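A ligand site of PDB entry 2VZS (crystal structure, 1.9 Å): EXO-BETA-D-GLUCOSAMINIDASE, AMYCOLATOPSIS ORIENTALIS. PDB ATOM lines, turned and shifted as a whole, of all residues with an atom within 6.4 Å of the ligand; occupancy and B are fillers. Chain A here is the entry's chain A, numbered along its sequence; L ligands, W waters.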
ATOM      1  N   ILE A 202      18.880 -24.521 -20.750  1.00  0.00           N
ATOM      2  CA  ILE A 202      19.507 -24.920 -22.047  1.00  0.00           C
ATOM      3  C   ILE A 202      18.538 -25.867 -22.759  1.00  0.00           C
ATOM      4  O   ILE A 202      17.406 -25.489 -23.031  1.00  0.00           O
ATOM      5  CB  ILE A 202      20.983 -25.452 -21.846  1.00  0.00           C
ATOM      6  CG1 ILE A 202      21.713 -24.531 -20.815  1.00  0.00           C
ATOM      7  CG2 ILE A 202      21.743 -25.555 -23.234  1.00  0.00           C
ATOM      8  CD1 ILE A 202      23.104 -24.986 -20.261  1.00  0.00           C
ATOM      9  N   ASP A 203      18.927 -27.106 -23.012  1.00  0.00           N
ATOM     10  CA  ASP A 203      18.011 -28.090 -23.648  1.00  0.00           C
ATOM     11  C   ASP A 203      17.952 -29.376 -22.798  1.00  0.00           C
ATOM     12  O   ASP A 203      17.588 -30.469 -23.282  1.00  0.00           O
ATOM     13  CB  ASP A 203      18.508 -28.408 -25.070  1.00  0.00           C
ATOM     14  CG  ASP A 203      19.953 -28.913 -25.078  1.00  0.00           C
ATOM     15  OD1 ASP A 203      20.578 -29.017 -23.992  1.00  0.00           O
ATOM     16  OD2 ASP A 203      20.473 -29.222 -26.153  1.00  0.00           O
ATOM     17  N   TRP A 204      18.285 -29.254 -21.514  1.00  0.00           N
ATOM     18  CA  TRP A 204      18.351 -30.442 -20.654  1.00  0.00           C
ATOM     19  C   TRP A 204      16.974 -31.084 -20.391  1.00  0.00           C
ATOM     20  O   TRP A 204      16.882 -32.303 -20.263  1.00  0.00           O
ATOM     21  CB  TRP A 204      19.034 -30.112 -19.336  1.00  0.00           C
ATOM     22  CG  TRP A 204      20.443 -29.547 -19.459  1.00  0.00           C
ATOM     23  CD1 TRP A 204      21.217 -29.456 -20.607  1.00  0.00           C
ATOM     24  CD2 TRP A 204      21.253 -29.038 -18.382  1.00  0.00           C
ATOM     25  NE1 TRP A 204      22.446 -28.888 -20.294  1.00  0.00           N
ATOM     26  CE2 TRP A 204      22.492 -28.623 -18.949  1.00  0.00           C
ATOM     27  CE3 TRP A 204      21.038 -28.848 -17.007  1.00  0.00           C
ATOM     28  CZ2 TRP A 204      23.519 -28.058 -18.173  1.00  0.00           C
ATOM     29  CZ3 TRP A 204      22.061 -28.299 -16.231  1.00  0.00           C
ATOM     30  CH2 TRP A 204      23.279 -27.886 -16.820  1.00  0.00           C
ATOM     31  N   ARG A 392      30.798 -32.132 -12.898  1.00  0.00           N
ATOM     32  CA  ARG A 392      30.834 -30.815 -13.488  1.00  0.00           C
ATOM     33  C   ARG A 392      29.502 -30.125 -13.219  1.00  0.00           C
ATOM     34  O   ARG A 392      28.452 -30.738 -13.362  1.00  0.00           O
ATOM     35  CB  ARG A 392      31.013 -30.944 -15.003  1.00  0.00           C
ATOM     36  CG  ARG A 392      31.129 -29.603 -15.674  1.00  0.00           C
ATOM     37  CD  ARG A 392      31.510 -29.705 -17.177  1.00  0.00           C
ATOM     38  NE  ARG A 392      31.243 -28.374 -17.772  1.00  0.00           N
ATOM     39  CZ  ARG A 392      30.799 -28.133 -19.002  1.00  0.00           C
ATOM     40  NH1 ARG A 392      30.586 -29.124 -19.864  1.00  0.00           N
ATOM     41  NH2 ARG A 392      30.566 -26.865 -19.366  1.00  0.00           N
ATOM     42  N   GLU A 394      27.690 -27.181 -14.898  1.00  0.00           N
ATOM     43  CA  GLU A 394      27.571 -26.175 -15.952  1.00  0.00           C
ATOM     44  C   GLU A 394      26.509 -25.195 -15.466  1.00  0.00           C
ATOM     45  O   GLU A 394      25.304 -25.455 -15.685  1.00  0.00           O
ATOM     46  CB  GLU A 394      27.211 -26.778 -17.329  1.00  0.00           C
ATOM     47  CG  GLU A 394      27.193 -25.609 -18.391  1.00  0.00           C
ATOM     48  CD  GLU A 394      26.853 -26.021 -19.812  1.00  0.00           C
ATOM     49  OE1 GLU A 394      26.327 -27.144 -20.013  1.00  0.00           O
ATOM     50  OE2 GLU A 394      27.055 -25.186 -20.745  1.00  0.00           O
ATOM     51  N   CYS A 419      26.484 -22.180 -20.769  1.00  0.00           N
ATOM     52  CA  CYS A 419      26.405 -21.693 -22.150  1.00  0.00           C
ATOM     53  C   CYS A 419      25.005 -21.215 -22.443  1.00  0.00           C
ATOM     54  O   CYS A 419      24.079 -21.350 -21.601  1.00  0.00           O
ATOM     55  CB  CYS A 419      26.696 -22.829 -23.144  1.00  0.00           C
ATOM     56  SG  CYS A 419      25.314 -24.023 -23.360  1.00  0.00           S
ATOM     57  N   CYS A 420      24.847 -20.732 -23.688  1.00  0.00           N
ATOM     58  CA  CYS A 420      23.532 -20.745 -24.350  1.00  0.00           C
ATOM     59  C   CYS A 420      22.438 -19.842 -23.736  1.00  0.00           C
ATOM     60  O   CYS A 420      21.237 -20.085 -23.927  1.00  0.00           O
ATOM     61  CB  CYS A 420      23.031 -22.216 -24.477  1.00  0.00           C
ATOM     62  SG  CYS A 420      24.339 -23.364 -25.060  1.00  0.00           S
ATOM     63  N   GLU A 431      23.370 -17.687 -31.181  1.00  0.00           N
ATOM     64  CA  GLU A 431      22.860 -18.514 -30.082  1.00  0.00           C
ATOM     65  C   GLU A 431      22.053 -17.657 -29.086  1.00  0.00           C
ATOM     66  O   GLU A 431      22.235 -16.447 -29.031  1.00  0.00           O
ATOM     67  CB  GLU A 431      24.014 -19.246 -29.382  1.00  0.00           C
ATOM     68  CG  GLU A 431      23.633 -19.929 -28.034  1.00  0.00           C
ATOM     69  CD  GLU A 431      22.809 -21.207 -28.182  1.00  0.00           C
ATOM     70  OE1 GLU A 431      21.570 -21.138 -28.354  1.00  0.00           O
ATOM     71  OE2 GLU A 431      23.428 -22.298 -28.101  1.00  0.00           O
ATOM     72  N   SER A 468      31.820 -21.589 -21.245  1.00  0.00           N
ATOM     73  CA  SER A 468      31.423 -22.938 -21.563  1.00  0.00           C
ATOM     74  C   SER A 468      31.608 -23.541 -22.999  1.00  0.00           C
ATOM     75  O   SER A 468      32.681 -24.033 -23.328  1.00  0.00           O
ATOM     76  CB  SER A 468      30.030 -23.253 -20.940  1.00  0.00           C
ATOM     77  OG  SER A 468      29.609 -24.605 -21.173  1.00  0.00           O
ATOM     78  N   ASP A 469      30.617 -23.508 -23.891  1.00  0.00           N
ATOM     79  CA  ASP A 469      30.646 -23.022 -25.302  1.00  0.00           C
ATOM     80  C   ASP A 469      31.640 -21.990 -25.791  1.00  0.00           C
ATOM     81  O   ASP A 469      32.602 -22.340 -26.439  1.00  0.00           O
ATOM     82  CB  ASP A 469      29.252 -22.879 -25.905  1.00  0.00           C
ATOM     83  CG  ASP A 469      28.372 -24.106 -25.677  1.00  0.00           C
ATOM     84  OD1 ASP A 469      28.622 -24.925 -24.752  1.00  0.00           O
ATOM     85  OD2 ASP A 469      27.370 -24.210 -26.415  1.00  0.00           O
ATOM     86  N   ALA A 497      34.785 -24.951 -22.000  1.00  0.00           N
ATOM     87  CA  ALA A 497      34.668 -26.427 -22.096  1.00  0.00           C
ATOM     88  C   ALA A 497      34.789 -26.910 -23.549  1.00  0.00           C
ATOM     89  O   ALA A 497      35.019 -28.117 -23.813  1.00  0.00           O
ATOM     90  CB  ALA A 497      33.341 -26.934 -21.439  1.00  0.00           C
ATOM     91  N   MET A 512      34.520 -29.975 -27.241  1.00  0.00           N
ATOM     92  CA  MET A 512      33.095 -30.124 -27.216  1.00  0.00           C
ATOM     93  C   MET A 512      32.656 -30.406 -28.649  1.00  0.00           C
ATOM     94  O   MET A 512      32.160 -29.523 -29.337  1.00  0.00           O
ATOM     95  CB  MET A 512      32.421 -28.838 -26.678  1.00  0.00           C
ATOM     96  CG  MET A 512      30.879 -28.944 -26.521  1.00  0.00           C
ATOM     97  SD  MET A 512      30.182 -27.352 -26.012  1.00  0.00           S
ATOM     98  CE  MET A 512      31.086 -27.167 -24.447  1.00  0.00           C
ATOM     99  N   TYR A 516      25.797 -36.274 -28.572  1.00  0.00           N
ATOM    100  CA  TYR A 516      24.788 -36.145 -27.498  1.00  0.00           C
ATOM    101  C   TYR A 516      23.634 -37.065 -27.861  1.00  0.00           C
ATOM    102  O   TYR A 516      22.561 -36.992 -27.271  1.00  0.00           O
ATOM    103  CB  TYR A 516      24.244 -34.726 -27.348  1.00  0.00           C
ATOM    104  CG  TYR A 516      25.306 -33.691 -27.039  1.00  0.00           C
ATOM    105  CD1 TYR A 516      25.724 -33.429 -25.685  1.00  0.00           C
ATOM    106  CD2 TYR A 516      25.927 -32.978 -28.076  1.00  0.00           C
ATOM    107  CE1 TYR A 516      26.742 -32.473 -25.417  1.00  0.00           C
ATOM    108  CE2 TYR A 516      26.929 -32.035 -27.816  1.00  0.00           C
ATOM    109  CZ  TYR A 516      27.328 -31.774 -26.484  1.00  0.00           C
ATOM    110  OH  TYR A 516      28.326 -30.819 -26.239  1.00  0.00           O
ATOM    111  N   GLU A 541      31.780 -32.763 -22.028  1.00  0.00           N
ATOM    112  CA  GLU A 541      30.343 -33.113 -22.023  1.00  0.00           C
ATOM    113  C   GLU A 541      29.958 -33.933 -23.258  1.00  0.00           C
ATOM    114  O   GLU A 541      29.760 -33.386 -24.345  1.00  0.00           O
ATOM    115  CB  GLU A 541      29.488 -31.856 -21.970  1.00  0.00           C
ATOM    116  CG  GLU A 541      29.977 -30.758 -22.848  1.00  0.00           C
ATOM    117  CD  GLU A 541      28.962 -29.658 -22.954  1.00  0.00           C
ATOM    118  OE1 GLU A 541      29.090 -28.653 -22.205  1.00  0.00           O
ATOM    119  OE2 GLU A 541      28.046 -29.778 -23.821  1.00  0.00           O
ATOM    120  N   SER A 580      14.273 -28.992 -26.909  1.00  0.00           N
ATOM    121  CA  SER A 580      15.024 -28.849 -28.167  1.00  0.00           C
ATOM    122  C   SER A 580      14.398 -29.664 -29.282  1.00  0.00           C
ATOM    123  O   SER A 580      14.122 -30.848 -29.117  1.00  0.00           O
ATOM    124  CB  SER A 580      16.460 -29.352 -27.998  1.00  0.00           C
ATOM    125  OG  SER A 580      17.233 -29.081 -29.140  1.00  0.00           O
ATOM    126  N   PHE A 583      16.517 -32.814 -29.922  1.00  0.00           N
ATOM    127  CA  PHE A 583      16.441 -33.917 -28.954  1.00  0.00           C
ATOM    128  C   PHE A 583      15.036 -34.094 -28.451  1.00  0.00           C
ATOM    129  O   PHE A 583      14.820 -34.469 -27.299  1.00  0.00           O
ATOM    130  CB  PHE A 583      17.415 -33.698 -27.790  1.00  0.00           C
ATOM    131  CG  PHE A 583      18.837 -33.398 -28.233  1.00  0.00           C
ATOM    132  CD1 PHE A 583      19.572 -34.352 -28.960  1.00  0.00           C
ATOM    133  CD2 PHE A 583      19.414 -32.190 -27.948  1.00  0.00           C
ATOM    134  CE1 PHE A 583      20.878 -34.085 -29.388  1.00  0.00           C
ATOM    135  CE2 PHE A 583      20.727 -31.918 -28.347  1.00  0.00           C
ATOM    136  CZ  PHE A 583      21.458 -32.890 -29.087  1.00  0.00           C
ATOM    137  N   TRP A 642      27.458 -36.840 -20.273  1.00  0.00           N
ATOM    138  CA  TRP A 642      26.289 -35.936 -20.358  1.00  0.00           C
ATOM    139  C   TRP A 642      24.986 -36.770 -20.209  1.00  0.00           C
ATOM    140  O   TRP A 642      24.545 -37.375 -21.181  1.00  0.00           O
ATOM    141  CB  TRP A 642      26.326 -35.150 -21.704  1.00  0.00           C
ATOM    142  CG  TRP A 642      25.782 -33.732 -21.568  1.00  0.00           C
ATOM    143  CD1 TRP A 642      24.711 -33.177 -22.213  1.00  0.00           C
ATOM    144  CD2 TRP A 642      26.289 -32.734 -20.682  1.00  0.00           C
ATOM    145  NE1 TRP A 642      24.519 -31.893 -21.773  1.00  0.00           N
ATOM    146  CE2 TRP A 642      25.475 -31.596 -20.820  1.00  0.00           C
ATOM    147  CE3 TRP A 642      27.355 -32.714 -19.737  1.00  0.00           C
ATOM    148  CZ2 TRP A 642      25.708 -30.404 -20.087  1.00  0.00           C
ATOM    149  CZ3 TRP A 642      27.579 -31.532 -18.983  1.00  0.00           C
ATOM    150  CH2 TRP A 642      26.745 -30.390 -19.179  1.00  0.00           C
ATOM    151  N   MET A 643      24.365 -36.849 -19.024  1.00  0.00           N
ATOM    152  CA  MET A 643      24.742 -36.128 -17.779  1.00  0.00           C
ATOM    153  C   MET A 643      24.714 -37.150 -16.635  1.00  0.00           C
ATOM    154  O   MET A 643      24.167 -38.249 -16.796  1.00  0.00           O
ATOM    155  CB  MET A 643      23.732 -34.971 -17.504  1.00  0.00           C
ATOM    156  CG  MET A 643      23.889 -33.844 -18.553  1.00  0.00           C
ATOM    157  SD  MET A 643      22.919 -32.371 -18.368  1.00  0.00           S
ATOM    158  CE  MET A 643      23.577 -31.733 -16.811  1.00  0.00           C
ATOM    159  N   TRP A 653      20.218 -38.484 -21.093  1.00  0.00           N
ATOM    160  CA  TRP A 653      21.323 -37.759 -20.469  1.00  0.00           C
ATOM    161  C   TRP A 653      21.298 -37.943 -18.952  1.00  0.00           C
ATOM    162  O   TRP A 653      21.240 -36.981 -18.205  1.00  0.00           O
ATOM    163  CB  TRP A 653      21.279 -36.249 -20.810  1.00  0.00           C
ATOM    164  CG  TRP A 653      21.398 -35.917 -22.293  1.00  0.00           C
ATOM    165  CD1 TRP A 653      21.752 -36.778 -23.324  1.00  0.00           C
ATOM    166  CD2 TRP A 653      21.212 -34.633 -22.895  1.00  0.00           C
ATOM    167  NE1 TRP A 653      21.735 -36.099 -24.534  1.00  0.00           N
ATOM    168  CE2 TRP A 653      21.417 -34.790 -24.294  1.00  0.00           C
ATOM    169  CE3 TRP A 653      20.882 -33.355 -22.386  1.00  0.00           C
ATOM    170  CZ2 TRP A 653      21.311 -33.723 -25.193  1.00  0.00           C
ATOM    171  CZ3 TRP A 653      20.761 -32.272 -23.308  1.00  0.00           C
ATOM    172  CH2 TRP A 653      20.988 -32.465 -24.675  1.00  0.00           C
ATOM    173  N   TRP A 781      26.766 -32.095 -35.638  1.00  0.00           N
ATOM    174  CA  TRP A 781      27.378 -31.645 -34.401  1.00  0.00           C
ATOM    175  C   TRP A 781      27.093 -32.551 -33.200  1.00  0.00           C
ATOM    176  O   TRP A 781      27.861 -32.591 -32.243  1.00  0.00           O
ATOM    177  CB  TRP A 781      26.968 -30.206 -34.095  1.00  0.00           C
ATOM    178  CG  TRP A 781      25.496 -30.027 -33.755  1.00  0.00           C
ATOM    179  CD1 TRP A 781      24.444 -29.796 -34.625  1.00  0.00           C
ATOM    180  CD2 TRP A 781      24.932 -30.017 -32.429  1.00  0.00           C
ATOM    181  NE1 TRP A 781      23.276 -29.650 -33.910  1.00  0.00           N
ATOM    182  CE2 TRP A 781      23.542 -29.766 -32.569  1.00  0.00           C
ATOM    183  CE3 TRP A 781      25.470 -30.168 -31.147  1.00  0.00           C
ATOM    184  CZ2 TRP A 781      22.678 -29.688 -31.456  1.00  0.00           C
ATOM    185  CZ3 TRP A 781      24.617 -30.064 -30.042  1.00  0.00           C
ATOM    186  CH2 TRP A 781      23.243 -29.825 -30.209  1.00  0.00           C
HETATM  187  C1  LIG L   1      26.456 -27.905 -25.275  1.00  0.00           C
HETATM  188  C2  LIG L   1      26.035 -27.315 -23.909  1.00  0.00           C
HETATM  189  C3  LIG L   1      25.138 -28.275 -23.077  1.00  0.00           C
HETATM  190  C4  LIG L   1      24.092 -28.888 -24.008  1.00  0.00           C
HETATM  191  C5  LIG L   1      24.783 -29.662 -25.171  1.00  0.00           C
HETATM  192  C6  LIG L   1      23.799 -30.299 -26.124  1.00  0.00           C
HETATM  193  N1  LIG L   1      27.214 -26.781 -23.173  1.00  0.00           N
HETATM  194  O1  LIG L   1      26.521 -26.784 -26.145  1.00  0.00           O
HETATM  195  O2  LIG L   1      24.464 -27.598 -21.987  1.00  0.00           O
HETATM  196  O3  LIG L   1      23.201 -29.726 -23.301  1.00  0.00           O
HETATM  197  O4  LIG L   1      25.433 -28.613 -25.958  1.00  0.00           O
HETATM  198  O5  LIG L   1      23.053 -29.254 -26.771  1.00  0.00           O
HETATM  199  O   HOH W   1      26.794 -26.552 -29.032  1.00  0.00           O
HETATM  200  O   HOH W   2      23.599 -26.849 -27.734  1.00  0.00           O
HETATM  201  O   HOH W   3      27.908 -28.945 -28.470  1.00  0.00           O
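Residues that only touch the ligand: Ile 202 (3.4 Å), Ser 468 (3.8 Å), Tyr 516 (3.4 Å), Phe 583 (3.9 Å), Trp 653 (3.5 Å) and Trp 781 (3.5 Å).
Hydrophobic or aromatic side chains that line the ligand: Ile 202, Trp 204, Met 512, Tyr 516, Phe 583, Trp 642, Trp 653 and Trp 781.
The side-chain carboxylate of Glu 541 lies within hydrogen-bond range of the side-chain hydroxyl of Tyr 516 (2.6 Å).
The side-chain carboxylate (OE1) of Glu 541 lies within salt-bridge range of the guanidinium group (NH1) of Arg 392 (2.8 Å).
NE1 of Trp 642 sits close to SD of Met 643.
The side-chain sulfur (SG) of Cys 420 forms a disulfide with the side-chain sulfur (SG) of Cys 419, at 2.1 Å.
O of Tyr 516 is in hydrogen-bond range of NE1 of Trp 653, 3.0 Å away.
The backbone carbonyl oxygen (O) of Trp 653 is in hydrogen-bond range of the backbone NH (N) of Met 643.
OG of Ser 468 lies within hydrogen-bond range of NH2 of Arg 392 (3.0 Å).
O of Ser 468 lies within hydrogen-bond range of N of Ala 497 (2.7 Å).
The side-chain carboxylate (OD2) of Asp 203 sits at hydrogen-bond distance from an oxygen (O5) of the ligand (2.7 Å).
OD1 of Asp 469 lies within salt-bridge range of N1 of the ligand (2.8 Å).
N1 of the ligand is in salt-bridge range of OE2 of Glu 394.
N1 of the ligand is in salt-bridge range of OE1 of Glu 541, at 2.8 Å.
NE1 of Trp 204 sits at hydrogen-bond distance from O2 of the ligand, at 2.9 Å.
NE1 of Trp 642 sits at hydrogen-bond distance from O3 of the ligand.
A nitrogen (N1) of the ligand lies within hydrogen-bond range of the side-chain sulfur (SG) of Cys 419 (3.4 Å).
O1 of the ligand lies within hydrogen-bond range of SD of Met 512.
Water W3 lies within hydrogen-bond range of the side-chain hydroxyl of Tyr 516 (2.9 Å), an oxygen (O1) of the ligand (3.5 Å) and the side-chain sulfur of Met 512 (3.7 Å).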
